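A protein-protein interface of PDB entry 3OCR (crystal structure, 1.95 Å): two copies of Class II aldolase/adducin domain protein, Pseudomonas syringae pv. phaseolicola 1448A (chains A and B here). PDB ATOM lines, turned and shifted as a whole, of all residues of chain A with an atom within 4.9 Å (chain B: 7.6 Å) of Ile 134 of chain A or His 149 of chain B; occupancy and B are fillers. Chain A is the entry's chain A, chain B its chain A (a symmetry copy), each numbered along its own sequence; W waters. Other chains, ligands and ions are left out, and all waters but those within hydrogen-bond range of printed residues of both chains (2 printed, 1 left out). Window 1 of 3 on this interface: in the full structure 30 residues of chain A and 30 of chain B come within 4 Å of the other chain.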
ATOM      1  N   ASP A  52      17.273   7.202 -15.278  1.00  0.00           N
ATOM      2  CA  ASP A  52      17.577   8.339 -16.117  1.00  0.00           C
ATOM      3  C   ASP A  52      18.354   9.312 -15.210  1.00  0.00           C
ATOM      4  O   ASP A  52      17.867  10.377 -14.811  1.00  0.00           O
ATOM      5  CB  ASP A  52      16.258   8.900 -16.707  1.00  0.00           C
ATOM      6  CG  ASP A  52      16.430  10.222 -17.419  1.00  0.00           C
ATOM      7  OD1 ASP A  52      17.523  10.482 -17.954  1.00  0.00           O
ATOM      8  OD2 ASP A  52      15.449  10.999 -17.454  1.00  0.00           O
ATOM      9  N   HIS A 129      11.834   6.526 -17.085  1.00  0.00           N
ATOM     10  CA  HIS A 129      12.190   7.058 -18.394  1.00  0.00           C
ATOM     11  C   HIS A 129      13.209   6.148 -19.049  1.00  0.00           C
ATOM     12  O   HIS A 129      14.375   6.518 -19.167  1.00  0.00           O
ATOM     13  CB  HIS A 129      12.862   8.421 -18.272  1.00  0.00           C
ATOM     14  CG  HIS A 129      11.954   9.542 -17.885  1.00  0.00           C
ATOM     15  ND1 HIS A 129      12.444  10.778 -17.520  1.00  0.00           N
ATOM     16  CD2 HIS A 129      10.604   9.635 -17.821  1.00  0.00           C
ATOM     17  CE1 HIS A 129      11.436  11.581 -17.231  1.00  0.00           C
ATOM     18  NE2 HIS A 129      10.309  10.911 -17.404  1.00  0.00           N
ATOM     19  N   THR A 130      12.803   4.963 -19.467  1.00  0.00           N
ATOM     20  CA  THR A 130      13.721   4.020 -20.086  1.00  0.00           C
ATOM     21  C   THR A 130      13.663   4.180 -21.584  1.00  0.00           C
ATOM     22  O   THR A 130      12.663   4.672 -22.110  1.00  0.00           O
ATOM     23  CB  THR A 130      13.316   2.539 -19.767  1.00  0.00           C
ATOM     24  OG1 THR A 130      12.007   2.261 -20.320  1.00  0.00           O
ATOM     25  CG2 THR A 130      13.340   2.292 -18.264  1.00  0.00           C
ATOM     26  N   ARG A 131      14.726   3.754 -22.272  1.00  0.00           N
ATOM     27  CA  ARG A 131      14.777   3.758 -23.729  1.00  0.00           C
ATOM     28  C   ARG A 131      13.523   3.160 -24.375  1.00  0.00           C
ATOM     29  O   ARG A 131      12.876   3.795 -25.216  1.00  0.00           O
ATOM     30  CB  ARG A 131      16.030   3.001 -24.192  1.00  0.00           C
ATOM     31  CG  ARG A 131      16.180   2.825 -25.684  1.00  0.00           C
ATOM     32  CD  ARG A 131      17.186   1.708 -25.992  1.00  0.00           C
ATOM     33  NE  ARG A 131      16.737   0.426 -25.449  1.00  0.00           N
ATOM     34  CZ  ARG A 131      17.464  -0.373 -24.670  1.00  0.00           C
ATOM     35  NH1 ARG A 131      18.706  -0.037 -24.339  1.00  0.00           N
ATOM     36  NH2 ARG A 131      16.942  -1.517 -24.232  1.00  0.00           N
ATOM     37  N   ASP A 132      13.180   1.930 -24.000  1.00  0.00           N
ATOM     38  CA  ASP A 132      12.082   1.242 -24.689  1.00  0.00           C
ATOM     39  C   ASP A 132      10.677   1.617 -24.183  1.00  0.00           C
ATOM     40  O   ASP A 132       9.710   1.644 -24.969  1.00  0.00           O
ATOM     41  CB  ASP A 132      12.306  -0.272 -24.694  1.00  0.00           C
ATOM     42  CG  ASP A 132      13.555  -0.677 -25.482  1.00  0.00           C
ATOM     43  OD1 ASP A 132      14.060   0.117 -26.317  1.00  0.00           O
ATOM     44  OD2 ASP A 132      14.061  -1.784 -25.225  1.00  0.00           O
ATOM     45  N   GLY A 133      10.572   1.938 -22.906  1.00  0.00           N
ATOM     46  CA  GLY A 133       9.318   2.508 -22.327  1.00  0.00           C
ATOM     47  C   GLY A 133       8.905   3.829 -22.985  1.00  0.00           C
ATOM     48  O   GLY A 133       7.738   4.004 -23.425  1.00  0.00           O
ATOM     49  N   ILE A 134       9.858   4.759 -23.106  1.00  0.00           N
ATOM     50  CA  ILE A 134       9.595   6.012 -23.807  1.00  0.00           C
ATOM     51  C   ILE A 134       9.304   5.737 -25.286  1.00  0.00           C
ATOM     52  O   ILE A 134       8.392   6.314 -25.856  1.00  0.00           O
ATOM     53  CB  ILE A 134      10.737   7.016 -23.629  1.00  0.00           C
ATOM     54  CG1 ILE A 134      10.989   7.282 -22.129  1.00  0.00           C
ATOM     55  CG2 ILE A 134      10.462   8.299 -24.392  1.00  0.00           C
ATOM     56  CD1 ILE A 134      12.201   8.109 -21.891  1.00  0.00           C
ATOM     57  N   ALA A 135      10.054   4.811 -25.892  1.00  0.00           N
ATOM     58  CA  ALA A 135       9.865   4.487 -27.299  1.00  0.00           C
ATOM     59  C   ALA A 135       8.434   4.013 -27.579  1.00  0.00           C
ATOM     60  O   ALA A 135       7.739   4.488 -28.527  1.00  0.00           O
ATOM     61  CB  ALA A 135      10.902   3.413 -27.729  1.00  0.00           C
ATOM     62  N   VAL A 136       7.987   3.054 -26.779  1.00  0.00           N
ATOM     63  CA  VAL A 136       6.581   2.622 -26.892  1.00  0.00           C
ATOM     64  C   VAL A 136       5.608   3.773 -26.610  1.00  0.00           C
ATOM     65  O   VAL A 136       4.591   3.924 -27.338  1.00  0.00           O
ATOM     66  CB  VAL A 136       6.243   1.365 -26.036  1.00  0.00           C
ATOM     67  CG1 VAL A 136       4.744   1.055 -26.164  1.00  0.00           C
ATOM     68  CG2 VAL A 136       7.057   0.131 -26.510  1.00  0.00           C
ATOM     69  N   SER A 137       5.910   4.575 -25.584  1.00  0.00           N
ATOM     70  CA  SER A 137       5.139   5.799 -25.308  1.00  0.00           C
ATOM     71  C   SER A 137       4.968   6.675 -26.551  1.00  0.00           C
ATOM     72  O   SER A 137       3.924   7.299 -26.719  1.00  0.00           O
ATOM     73  CB  SER A 137       5.792   6.648 -24.221  1.00  0.00           C
ATOM     74  OG  SER A 137       6.164   5.865 -23.098  1.00  0.00           O
ATOM     75  N   ALA A 138       6.006   6.737 -27.388  1.00  0.00           N
ATOM     76  CA  ALA A 138       6.051   7.681 -28.513  1.00  0.00           C
ATOM     77  C   ALA A 138       5.292   7.216 -29.756  1.00  0.00           C
ATOM     78  O   ALA A 138       5.283   7.918 -30.781  1.00  0.00           O
ATOM     79  CB  ALA A 138       7.498   7.991 -28.869  1.00  0.00           C
ATOM     80  N   ASN A 189       4.863  10.052 -25.105  1.00  0.00           N
ATOM     81  CA  ASN A 189       6.096  10.784 -25.376  1.00  0.00           C
ATOM     82  C   ASN A 189       6.869  11.073 -24.103  1.00  0.00           C
ATOM     83  O   ASN A 189       7.572  12.067 -24.022  1.00  0.00           O
ATOM     84  CB  ASN A 189       5.802  12.103 -26.081  1.00  0.00           C
ATOM     85  CG  ASN A 189       4.984  11.904 -27.343  1.00  0.00           C
ATOM     86  OD1 ASN A 189       3.789  12.152 -27.326  1.00  0.00           O
ATOM     87  ND2 ASN A 189       5.616  11.419 -28.430  1.00  0.00           N
ATOM     88  N   HIS A 190       6.701  10.260 -23.082  1.00  0.00           N
ATOM     89  CA  HIS A 190       7.242  10.704 -21.810  1.00  0.00           C
ATOM     90  C   HIS A 190       7.844   9.544 -21.056  1.00  0.00           C
ATOM     91  O   HIS A 190       9.004   9.637 -20.648  1.00  0.00           O
ATOM     92  CB  HIS A 190       6.158  11.491 -21.020  1.00  0.00           C
ATOM     93  CG  HIS A 190       6.609  12.001 -19.680  1.00  0.00           C
ATOM     94  ND1 HIS A 190       5.764  12.664 -18.816  1.00  0.00           N
ATOM     95  CD2 HIS A 190       7.808  11.930 -19.049  1.00  0.00           C
ATOM     96  CE1 HIS A 190       6.428  12.996 -17.721  1.00  0.00           C
ATOM     97  NE2 HIS A 190       7.668  12.549 -17.833  1.00  0.00           N
ATOM     98  N   GLY A 191       7.089   8.456 -20.884  1.00  0.00           N
ATOM     99  CA  GLY A 191       7.589   7.236 -20.219  1.00  0.00           C
ATOM    100  C   GLY A 191       6.469   6.401 -19.574  1.00  0.00           C
ATOM    101  O   GLY A 191       5.305   6.387 -20.040  1.00  0.00           O
ATOM    102  N   LEU B 143      16.920  15.227 -35.259  1.00  0.00           N
ATOM    103  CA  LEU B 143      16.327  14.897 -33.956  1.00  0.00           C
ATOM    104  C   LEU B 143      14.860  15.293 -33.904  1.00  0.00           C
ATOM    105  O   LEU B 143      14.528  16.461 -33.985  1.00  0.00           O
ATOM    106  CB  LEU B 143      17.113  15.559 -32.814  1.00  0.00           C
ATOM    107  CG  LEU B 143      16.699  15.216 -31.383  1.00  0.00           C
ATOM    108  CD1 LEU B 143      17.150  13.833 -30.940  1.00  0.00           C
ATOM    109  CD2 LEU B 143      17.203  16.295 -30.412  1.00  0.00           C
ATOM    110  N   LEU B 144      13.997  14.294 -33.722  1.00  0.00           N
ATOM    111  CA  LEU B 144      12.550  14.465 -33.781  1.00  0.00           C
ATOM    112  C   LEU B 144      11.985  14.927 -32.417  1.00  0.00           C
ATOM    113  O   LEU B 144      12.545  14.573 -31.372  1.00  0.00           O
ATOM    114  CB  LEU B 144      11.915  13.136 -34.240  1.00  0.00           C
ATOM    115  CG  LEU B 144      12.341  12.583 -35.623  1.00  0.00           C
ATOM    116  CD1 LEU B 144      11.837  11.146 -35.804  1.00  0.00           C
ATOM    117  CD2 LEU B 144      11.801  13.435 -36.762  1.00  0.00           C
ATOM    118  N   PRO B 145      10.897  15.726 -32.417  1.00  0.00           N
ATOM    119  CA  PRO B 145      10.298  16.136 -31.138  1.00  0.00           C
ATOM    120  C   PRO B 145       9.263  15.096 -30.611  1.00  0.00           C
ATOM    121  O   PRO B 145       8.059  15.332 -30.653  1.00  0.00           O
ATOM    122  CB  PRO B 145       9.649  17.474 -31.482  1.00  0.00           C
ATOM    123  CG  PRO B 145       9.235  17.353 -32.922  1.00  0.00           C
ATOM    124  CD  PRO B 145      10.206  16.348 -33.570  1.00  0.00           C
ATOM    125  N   ILE B 146       9.732  13.949 -30.141  1.00  0.00           N
ATOM    126  CA  ILE B 146       8.805  12.823 -29.822  1.00  0.00           C
ATOM    127  C   ILE B 146       8.977  12.284 -28.409  1.00  0.00           C
ATOM    128  O   ILE B 146       8.348  11.288 -28.026  1.00  0.00           O
ATOM    129  CB  ILE B 146       8.904  11.657 -30.856  1.00  0.00           C
ATOM    130  CG1 ILE B 146      10.359  11.247 -31.126  1.00  0.00           C
ATOM    131  CG2 ILE B 146       8.277  12.077 -32.180  1.00  0.00           C
ATOM    132  CD1 ILE B 146      10.952  10.347 -30.067  1.00  0.00           C
ATOM    133  N   SER B 147       9.831  12.936 -27.643  1.00  0.00           N
ATOM    134  CA  SER B 147      10.053  12.558 -26.257  1.00  0.00           C
ATOM    135  C   SER B 147      10.346  13.806 -25.438  1.00  0.00           C
ATOM    136  O   SER B 147      10.803  14.810 -25.970  1.00  0.00           O
ATOM    137  CB  SER B 147      11.208  11.563 -26.138  1.00  0.00           C
ATOM    138  OG  SER B 147      12.481  12.174 -26.429  1.00  0.00           O
ATOM    139  N   GLN B 148      10.111  13.757 -24.128  1.00  0.00           N
ATOM    140  CA  GLN B 148      10.484  14.891 -23.276  1.00  0.00           C
ATOM    141  C   GLN B 148      11.956  15.281 -23.477  1.00  0.00           C
ATOM    142  O   GLN B 148      12.313  16.461 -23.508  1.00  0.00           O
ATOM    143  CB  GLN B 148      10.242  14.560 -21.818  1.00  0.00           C
ATOM    144  CG  GLN B 148      10.606  15.693 -20.878  1.00  0.00           C
ATOM    145  CD  GLN B 148       9.893  15.575 -19.556  1.00  0.00           C
ATOM    146  OE1 GLN B 148      10.515  15.254 -18.523  1.00  0.00           O
ATOM    147  NE2 GLN B 148       8.581  15.812 -19.569  1.00  0.00           N
ATOM    148  N   HIS B 149      12.799  14.268 -23.603  1.00  0.00           N
ATOM    149  CA  HIS B 149      14.241  14.448 -23.745  1.00  0.00           C
ATOM    150  C   HIS B 149      14.642  15.165 -25.043  1.00  0.00           C
ATOM    151  O   HIS B 149      15.498  16.052 -25.021  1.00  0.00           O
ATOM    152  CB  HIS B 149      14.934  13.088 -23.623  1.00  0.00           C
ATOM    153  CG  HIS B 149      14.646  12.407 -22.327  1.00  0.00           C
ATOM    154  ND1 HIS B 149      13.397  11.903 -22.016  1.00  0.00           N
ATOM    155  CD2 HIS B 149      15.424  12.186 -21.242  1.00  0.00           C
ATOM    156  CE1 HIS B 149      13.428  11.382 -20.800  1.00  0.00           C
ATOM    157  NE2 HIS B 149      14.645  11.538 -20.311  1.00  0.00           N
ATOM    158  N   SER B 150      14.027  14.790 -26.166  1.00  0.00           N
ATOM    159  CA  SER B 150      14.314  15.459 -27.430  1.00  0.00           C
ATOM    160  C   SER B 150      13.646  16.841 -27.529  1.00  0.00           C
ATOM    161  O   SER B 150      14.233  17.764 -28.108  1.00  0.00           O
ATOM    162  CB  SER B 150      13.895  14.599 -28.626  1.00  0.00           C
ATOM    163  OG  SER B 150      12.520  14.302 -28.567  1.00  0.00           O
ATOM    164  N   ILE B 151      12.422  16.962 -26.989  1.00  0.00           N
ATOM    165  CA  ILE B 151      11.616  18.195 -27.105  1.00  0.00           C
ATOM    166  C   ILE B 151      12.302  19.320 -26.329  1.00  0.00           C
ATOM    167  O   ILE B 151      12.255  20.486 -26.731  1.00  0.00           O
ATOM    168  CB  ILE B 151      10.129  17.952 -26.654  1.00  0.00           C
ATOM    169  CG1 ILE B 151       9.430  17.002 -27.613  1.00  0.00           C
ATOM    170  CG2 ILE B 151       9.308  19.253 -26.529  1.00  0.00           C
ATOM    171  CD1 ILE B 151       8.103  16.369 -27.049  1.00  0.00           C
ATOM    172  N   ALA B 152      12.993  18.957 -25.246  1.00  0.00           N
ATOM    173  CA  ALA B 152      13.793  19.904 -24.490  1.00  0.00           C
ATOM    174  C   ALA B 152      14.904  20.594 -25.323  1.00  0.00           C
ATOM    175  O   ALA B 152      15.341  21.703 -24.990  1.00  0.00           O
ATOM    176  CB  ALA B 152      14.394  19.196 -23.241  1.00  0.00           C
ATOM    177  N   PHE B 153      15.361  19.938 -26.396  1.00  0.00           N
ATOM    178  CA  PHE B 153      16.315  20.547 -27.350  1.00  0.00           C
ATOM    179  C   PHE B 153      15.671  21.378 -28.472  1.00  0.00           C
ATOM    180  O   PHE B 153      16.376  21.900 -29.341  1.00  0.00           O
ATOM    181  CB  PHE B 153      17.209  19.449 -27.959  1.00  0.00           C
ATOM    182  CG  PHE B 153      18.271  18.975 -27.000  1.00  0.00           C
ATOM    183  CD1 PHE B 153      18.083  17.822 -26.245  1.00  0.00           C
ATOM    184  CD2 PHE B 153      19.415  19.730 -26.807  1.00  0.00           C
ATOM    185  CE1 PHE B 153      19.072  17.409 -25.314  1.00  0.00           C
ATOM    186  CE2 PHE B 153      20.408  19.317 -25.901  1.00  0.00           C
ATOM    187  CZ  PHE B 153      20.220  18.160 -25.169  1.00  0.00           C
ATOM    188  N   SER B 154      14.350  21.515 -28.466  1.00  0.00           N
ATOM    189  CA  SER B 154      13.708  22.241 -29.562  1.00  0.00           C
ATOM    190  C   SER B 154      14.220  23.685 -29.601  1.00  0.00           C
ATOM    191  O   SER B 154      14.218  24.382 -28.577  1.00  0.00           O
ATOM    192  CB  SER B 154      12.189  22.206 -29.427  1.00  0.00           C
ATOM    193  OG  SER B 154      11.581  22.973 -30.462  1.00  0.00           O
ATOM    194  N   ARG B 156      17.282  24.566 -29.903  1.00  0.00           N
ATOM    195  CA  ARG B 156      18.642  24.677 -29.357  1.00  0.00           C
ATOM    196  C   ARG B 156      19.727  24.092 -30.294  1.00  0.00           C
ATOM    197  O   ARG B 156      20.927  24.202 -30.011  1.00  0.00           O
ATOM    198  CB  ARG B 156      18.732  23.995 -27.990  1.00  0.00           C
ATOM    199  CG  ARG B 156      18.063  24.764 -26.834  1.00  0.00           C
ATOM    200  CD  ARG B 156      17.828  23.820 -25.659  1.00  0.00           C
ATOM    201  NE  ARG B 156      19.065  23.372 -24.987  1.00  0.00           N
ATOM    202  CZ  ARG B 156      19.139  22.327 -24.160  1.00  0.00           C
ATOM    203  NH1 ARG B 156      18.068  21.578 -23.914  1.00  0.00           N
ATOM    204  NH2 ARG B 156      20.294  22.017 -23.572  1.00  0.00           N
ATOM    205  N   HIS B 207      25.226  14.512 -22.375  1.00  0.00           N
ATOM    206  CA  HIS B 207      24.482  13.445 -21.700  1.00  0.00           C
ATOM    207  C   HIS B 207      23.007  13.409 -22.084  1.00  0.00           C
ATOM    208  O   HIS B 207      22.475  12.334 -22.385  1.00  0.00           O
ATOM    209  CB  HIS B 207      24.653  13.572 -20.183  1.00  0.00           C
ATOM    210  CG  HIS B 207      24.197  12.373 -19.400  1.00  0.00           C
ATOM    211  ND1 HIS B 207      24.206  12.348 -18.022  1.00  0.00           N
ATOM    212  CD2 HIS B 207      23.747  11.155 -19.789  1.00  0.00           C
ATOM    213  CE1 HIS B 207      23.774  11.174 -17.594  1.00  0.00           C
ATOM    214  NE2 HIS B 207      23.492  10.430 -18.647  1.00  0.00           N
ATOM    215  N   ALA B 208      22.351  14.566 -22.070  1.00  0.00           N
ATOM    216  CA  ALA B 208      20.944  14.640 -22.434  1.00  0.00           C
ATOM    217  C   ALA B 208      20.708  14.375 -23.898  1.00  0.00           C
ATOM    218  O   ALA B 208      19.723  13.721 -24.251  1.00  0.00           O
ATOM    219  CB  ALA B 208      20.339  15.994 -22.053  1.00  0.00           C
ATOM    220  N   LEU B 209      21.596  14.883 -24.753  1.00  0.00           N
ATOM    221  CA  LEU B 209      21.434  14.744 -26.191  1.00  0.00           C
ATOM    222  C   LEU B 209      21.631  13.278 -26.595  1.00  0.00           C
ATOM    223  O   LEU B 209      20.902  12.762 -27.441  1.00  0.00           O
ATOM    224  CB  LEU B 209      22.415  15.644 -26.951  1.00  0.00           C
ATOM    225  CG  LEU B 209      22.239  15.696 -28.481  1.00  0.00           C
ATOM    226  CD1 LEU B 209      20.803  16.135 -28.863  1.00  0.00           C
ATOM    227  CD2 LEU B 209      23.325  16.563 -29.169  1.00  0.00           C
ATOM    228  N   TYR B 211      21.172  10.638 -24.740  1.00  0.00           N
ATOM    229  CA  TYR B 211      19.969   9.904 -24.342  1.00  0.00           C
ATOM    230  C   TYR B 211      18.787  10.154 -25.285  1.00  0.00           C
ATOM    231  O   TYR B 211      18.070   9.225 -25.636  1.00  0.00           O
ATOM    232  CB  TYR B 211      19.561  10.218 -22.921  1.00  0.00           C
ATOM    233  CG  TYR B 211      18.689   9.109 -22.301  1.00  0.00           C
ATOM    234  CD1 TYR B 211      18.971   7.751 -22.529  1.00  0.00           C
ATOM    235  CD2 TYR B 211      17.607   9.418 -21.492  1.00  0.00           C
ATOM    236  CE1 TYR B 211      18.182   6.731 -21.950  1.00  0.00           C
ATOM    237  CE2 TYR B 211      16.822   8.417 -20.904  1.00  0.00           C
ATOM    238  CZ  TYR B 211      17.119   7.083 -21.128  1.00  0.00           C
ATOM    239  OH  TYR B 211      16.338   6.104 -20.553  1.00  0.00           O
ATOM    240  N   ALA B 212      18.560  11.407 -25.637  1.00  0.00           N
ATOM    241  CA  ALA B 212      17.490  11.722 -26.612  1.00  0.00           C
ATOM    242  C   ALA B 212      17.694  10.893 -27.879  1.00  0.00           C
ATOM    243  O   ALA B 212      16.741  10.323 -28.395  1.00  0.00           O
ATOM    244  CB  ALA B 212      17.449  13.220 -26.918  1.00  0.00           C
ATOM    245  N   CYS B 213      18.934  10.781 -28.361  1.00  0.00           N
ATOM    246  CA  CYS B 213      19.193   9.958 -29.528  1.00  0.00           C
ATOM    247  C   CYS B 213      18.941   8.468 -29.291  1.00  0.00           C
ATOM    248  O   CYS B 213      18.359   7.846 -30.152  1.00  0.00           O
ATOM    249  CB  CYS B 213      20.594  10.161 -30.122  1.00  0.00           C
ATOM    250  SG  CYS B 213      20.957  11.850 -30.656  1.00  0.00           S
ATOM    251  N   ILE B 215      16.776   7.111 -27.438  1.00  0.00           N
ATOM    252  CA  ILE B 215      15.375   6.933 -27.332  1.00  0.00           C
ATOM    253  C   ILE B 215      14.809   7.024 -28.765  1.00  0.00           C
ATOM    254  O   ILE B 215      13.912   6.263 -29.119  1.00  0.00           O
ATOM    255  CB  ILE B 215      14.732   8.077 -26.470  1.00  0.00           C
ATOM    256  CG1 ILE B 215      14.987   7.875 -24.978  1.00  0.00           C
ATOM    257  CG2 ILE B 215      13.231   8.174 -26.764  1.00  0.00           C
ATOM    258  CD1 ILE B 215      14.875   9.196 -24.180  1.00  0.00           C
ATOM    259  N   GLN B 216      15.343   7.927 -29.573  1.00  0.00           N
ATOM    260  CA  GLN B 216      14.772   8.122 -30.962  1.00  0.00           C
ATOM    261  C   GLN B 216      14.915   6.861 -31.832  1.00  0.00           C
ATOM    262  O   GLN B 216      14.008   6.505 -32.609  1.00  0.00           O
ATOM    263  CB  GLN B 216      15.500   9.226 -31.707  1.00  0.00           C
ATOM    264  CG  GLN B 216      14.893   9.424 -33.204  1.00  0.00           C
ATOM    265  CD  GLN B 216      15.286  10.766 -33.804  1.00  0.00           C
ATOM    266  OE1 GLN B 216      15.200  11.801 -33.142  1.00  0.00           O
ATOM    267  NE2 GLN B 216      15.725  10.757 -35.050  1.00  0.00           N
ATOM    268  N   ALA B 218      15.176   3.731 -30.890  1.00  0.00           N
ATOM    269  CA  ALA B 218      14.131   2.751 -30.440  1.00  0.00           C
ATOM    270  C   ALA B 218      12.724   3.145 -30.911  1.00  0.00           C
ATOM    271  O   ALA B 218      11.990   2.318 -31.521  1.00  0.00           O
ATOM    272  CB  ALA B 218      14.162   2.605 -28.934  1.00  0.00           C
ATOM    273  N   ALA B 219      12.354   4.404 -30.659  1.00  0.00           N
ATOM    274  CA  ALA B 219      10.992   4.925 -30.953  1.00  0.00           C
ATOM    275  C   ALA B 219      10.580   4.704 -32.389  1.00  0.00           C
ATOM    276  O   ALA B 219       9.421   4.299 -32.695  1.00  0.00           O
ATOM    277  CB  ALA B 219      10.907   6.448 -30.603  1.00  0.00           C
ATOM    278  N   LEU B 227       4.980   7.429 -35.224  1.00  0.00           N
ATOM    279  CA  LEU B 227       5.292   8.299 -34.107  1.00  0.00           C
ATOM    280  C   LEU B 227       4.164   9.257 -33.772  1.00  0.00           C
ATOM    281  O   LEU B 227       3.448   9.725 -34.668  1.00  0.00           O
ATOM    282  CB  LEU B 227       6.590   9.063 -34.372  1.00  0.00           C
ATOM    283  CG  LEU B 227       7.866   8.242 -34.524  1.00  0.00           C
ATOM    284  CD1 LEU B 227       8.986   9.155 -34.943  1.00  0.00           C
ATOM    285  CD2 LEU B 227       8.233   7.551 -33.239  1.00  0.00           C
ATOM    286  N   VAL B 238       7.571  23.432 -23.562  1.00  0.00           N
ATOM    287  CA  VAL B 238       8.790  22.787 -23.089  1.00  0.00           C
ATOM    288  C   VAL B 238      10.014  23.663 -23.375  1.00  0.00           C
ATOM    289  O   VAL B 238      10.965  23.718 -22.558  1.00  0.00           O
ATOM    290  CB  VAL B 238       8.938  21.361 -23.644  1.00  0.00           C
ATOM    291  CG1 VAL B 238      10.316  20.754 -23.264  1.00  0.00           C
ATOM    292  CG2 VAL B 238       7.806  20.472 -23.104  1.00  0.00           C
HETATM  293  O   HOH W   1      17.154   3.123 -21.074  1.00  0.00           O
HETATM  294  O   HOH W   2      10.560  11.477 -22.170  1.00  0.00           O
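Asp 52 of chain A touches Tyr 211 of chain B (OD1 to CE2, 3.7 Å). Thr 130 of chain A touches Tyr 211 of chain B. Arg 131 of chain A touches Ala 218 of chain B (CG to CB, 3.8 Å). CB of Ala 218 of chain B touches OD1 of Asp 132 of chain A, at 3.6 Å. CG2 of Ile 134 of chain A touches CB of Ser 147 of chain B (3.8 Å). Ile 134 of chain A touches His 149 of chain B (CD1 to CE1, 3.7 Å). Ala 135 of chain A touches Ala 218 of chain B. Ala 138 of chain A touches Ile 146 of chain B. Ala 138 of chain A touches Leu 227 of chain B (O to CA, 3.3 Å). Gln 148 of chain B touches His 190 of chain A (NE2 to NE2, 3.8 Å).
Of the 25 printed residues of chain B, 9 touch a printed residue of chain A. Hydrophobic or aromatic side chains of chain B that line the printed part of chain A: His 149, Tyr 211, Ile 215, Ala 218, Ala 219 and Leu 227. Of the 14 printed residues of chain A, 10 touch a printed residue of chain B. Hydrophobic or aromatic side chains of chain A within 4 Å of the printed part of chain B: His 129, Ile 134, Ala 135, Ala 138 and His 190.
Of the printed residues of chain A, His 149 of chain B touches Asp 52 (3.0 Å), His 129 (3.5 Å) and Ile 134 (3.7 Å). No residue of chain B comes within 4 Å of Gly 133 of chain A. Printed residues of chain B within 4 Å of Asn 189 of chain A: Ile 146, Ser 147 and Gln 148. Of the printed residues of chain B, Asp 132 of chain A touches Ala 218. Of the printed residues of chain B, Thr 130 of chain A touches Tyr 211 (3.4 Å). Ser 150 of chain B touches none of the printed residues of chain A. Pro 145 of chain B touches none of the printed residues of chain A. The nearest residue of chain A that does not touch His 149 of chain B is His 190 of chain A (4.8 Å). The nearest printed residue of chain B that does not touch Asp 52 of chain A is His 207 of chain B (6.0 Å).
Water W1 bridges the backbone NH (N) of Arg 131 of chain A (2.8 Å) and the side-chain hydroxyl (OH) of Tyr 211 of chain B (3.1 Å). Water W2 lies within hydrogen-bond range of O of His 190 of chain A, ND1 of His 149 of chain B and N of Gln 148 of chain B.
No position is printed for both chains.
NE of Arg 131 of chain A lies within salt-bridge range of OD1 of Asp 132 of chain A, 2.8 Å away. The backbone carbonyl oxygen of Ser 137 of chain A is in hydrogen-bond range of the backbone NH of Asn 189 of chain A (3.3 Å). The backbone NH (N) of Gly 133 of chain A is in hydrogen-bond range of the side-chain hydroxyl (OG1) of Thr 130 of chain A (3.0 Å). The side-chain hydroxyl (OG) of Ser 150 of chain B lies within hydrogen-bond range of the backbone NH (N) of Ile 146 of chain B (3.2 Å). ND1 of His 129 of chain A sits at hydrogen-bond distance from OD2 of Asp 52 of chain A, at 3.0 Å. NE2 of His 129 of chain A lies within hydrogen-bond range of NE2 of His 190 of chain A, at 3.1 Å.
The backbone carbonyl oxygen of His 129 of chain A is in hydrogen-bond range of the side-chain hydroxyl of Tyr 211 of chain B (2.4 Å). NE2 of His 149 of chain B lies within hydrogen-bond range of OD2 of Asp 52 of chain A (3.0 Å). The backbone carbonyl oxygen (O) of Ile 146 of chain B is in hydrogen-bond range of the side-chain amide nitrogen (ND2) of Asn 189 of chain A, at 2.8 Å. The side-chain hydroxyl of Tyr 211 of chain B lies within hydrogen-bond range of the backbone NH of Arg 131 of chain A (3.3 Å). The backbone carbonyl oxygen (O) of Asn 189 of chain A lies within hydrogen-bond range of the backbone NH (N) of Gln 148 of chain B.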
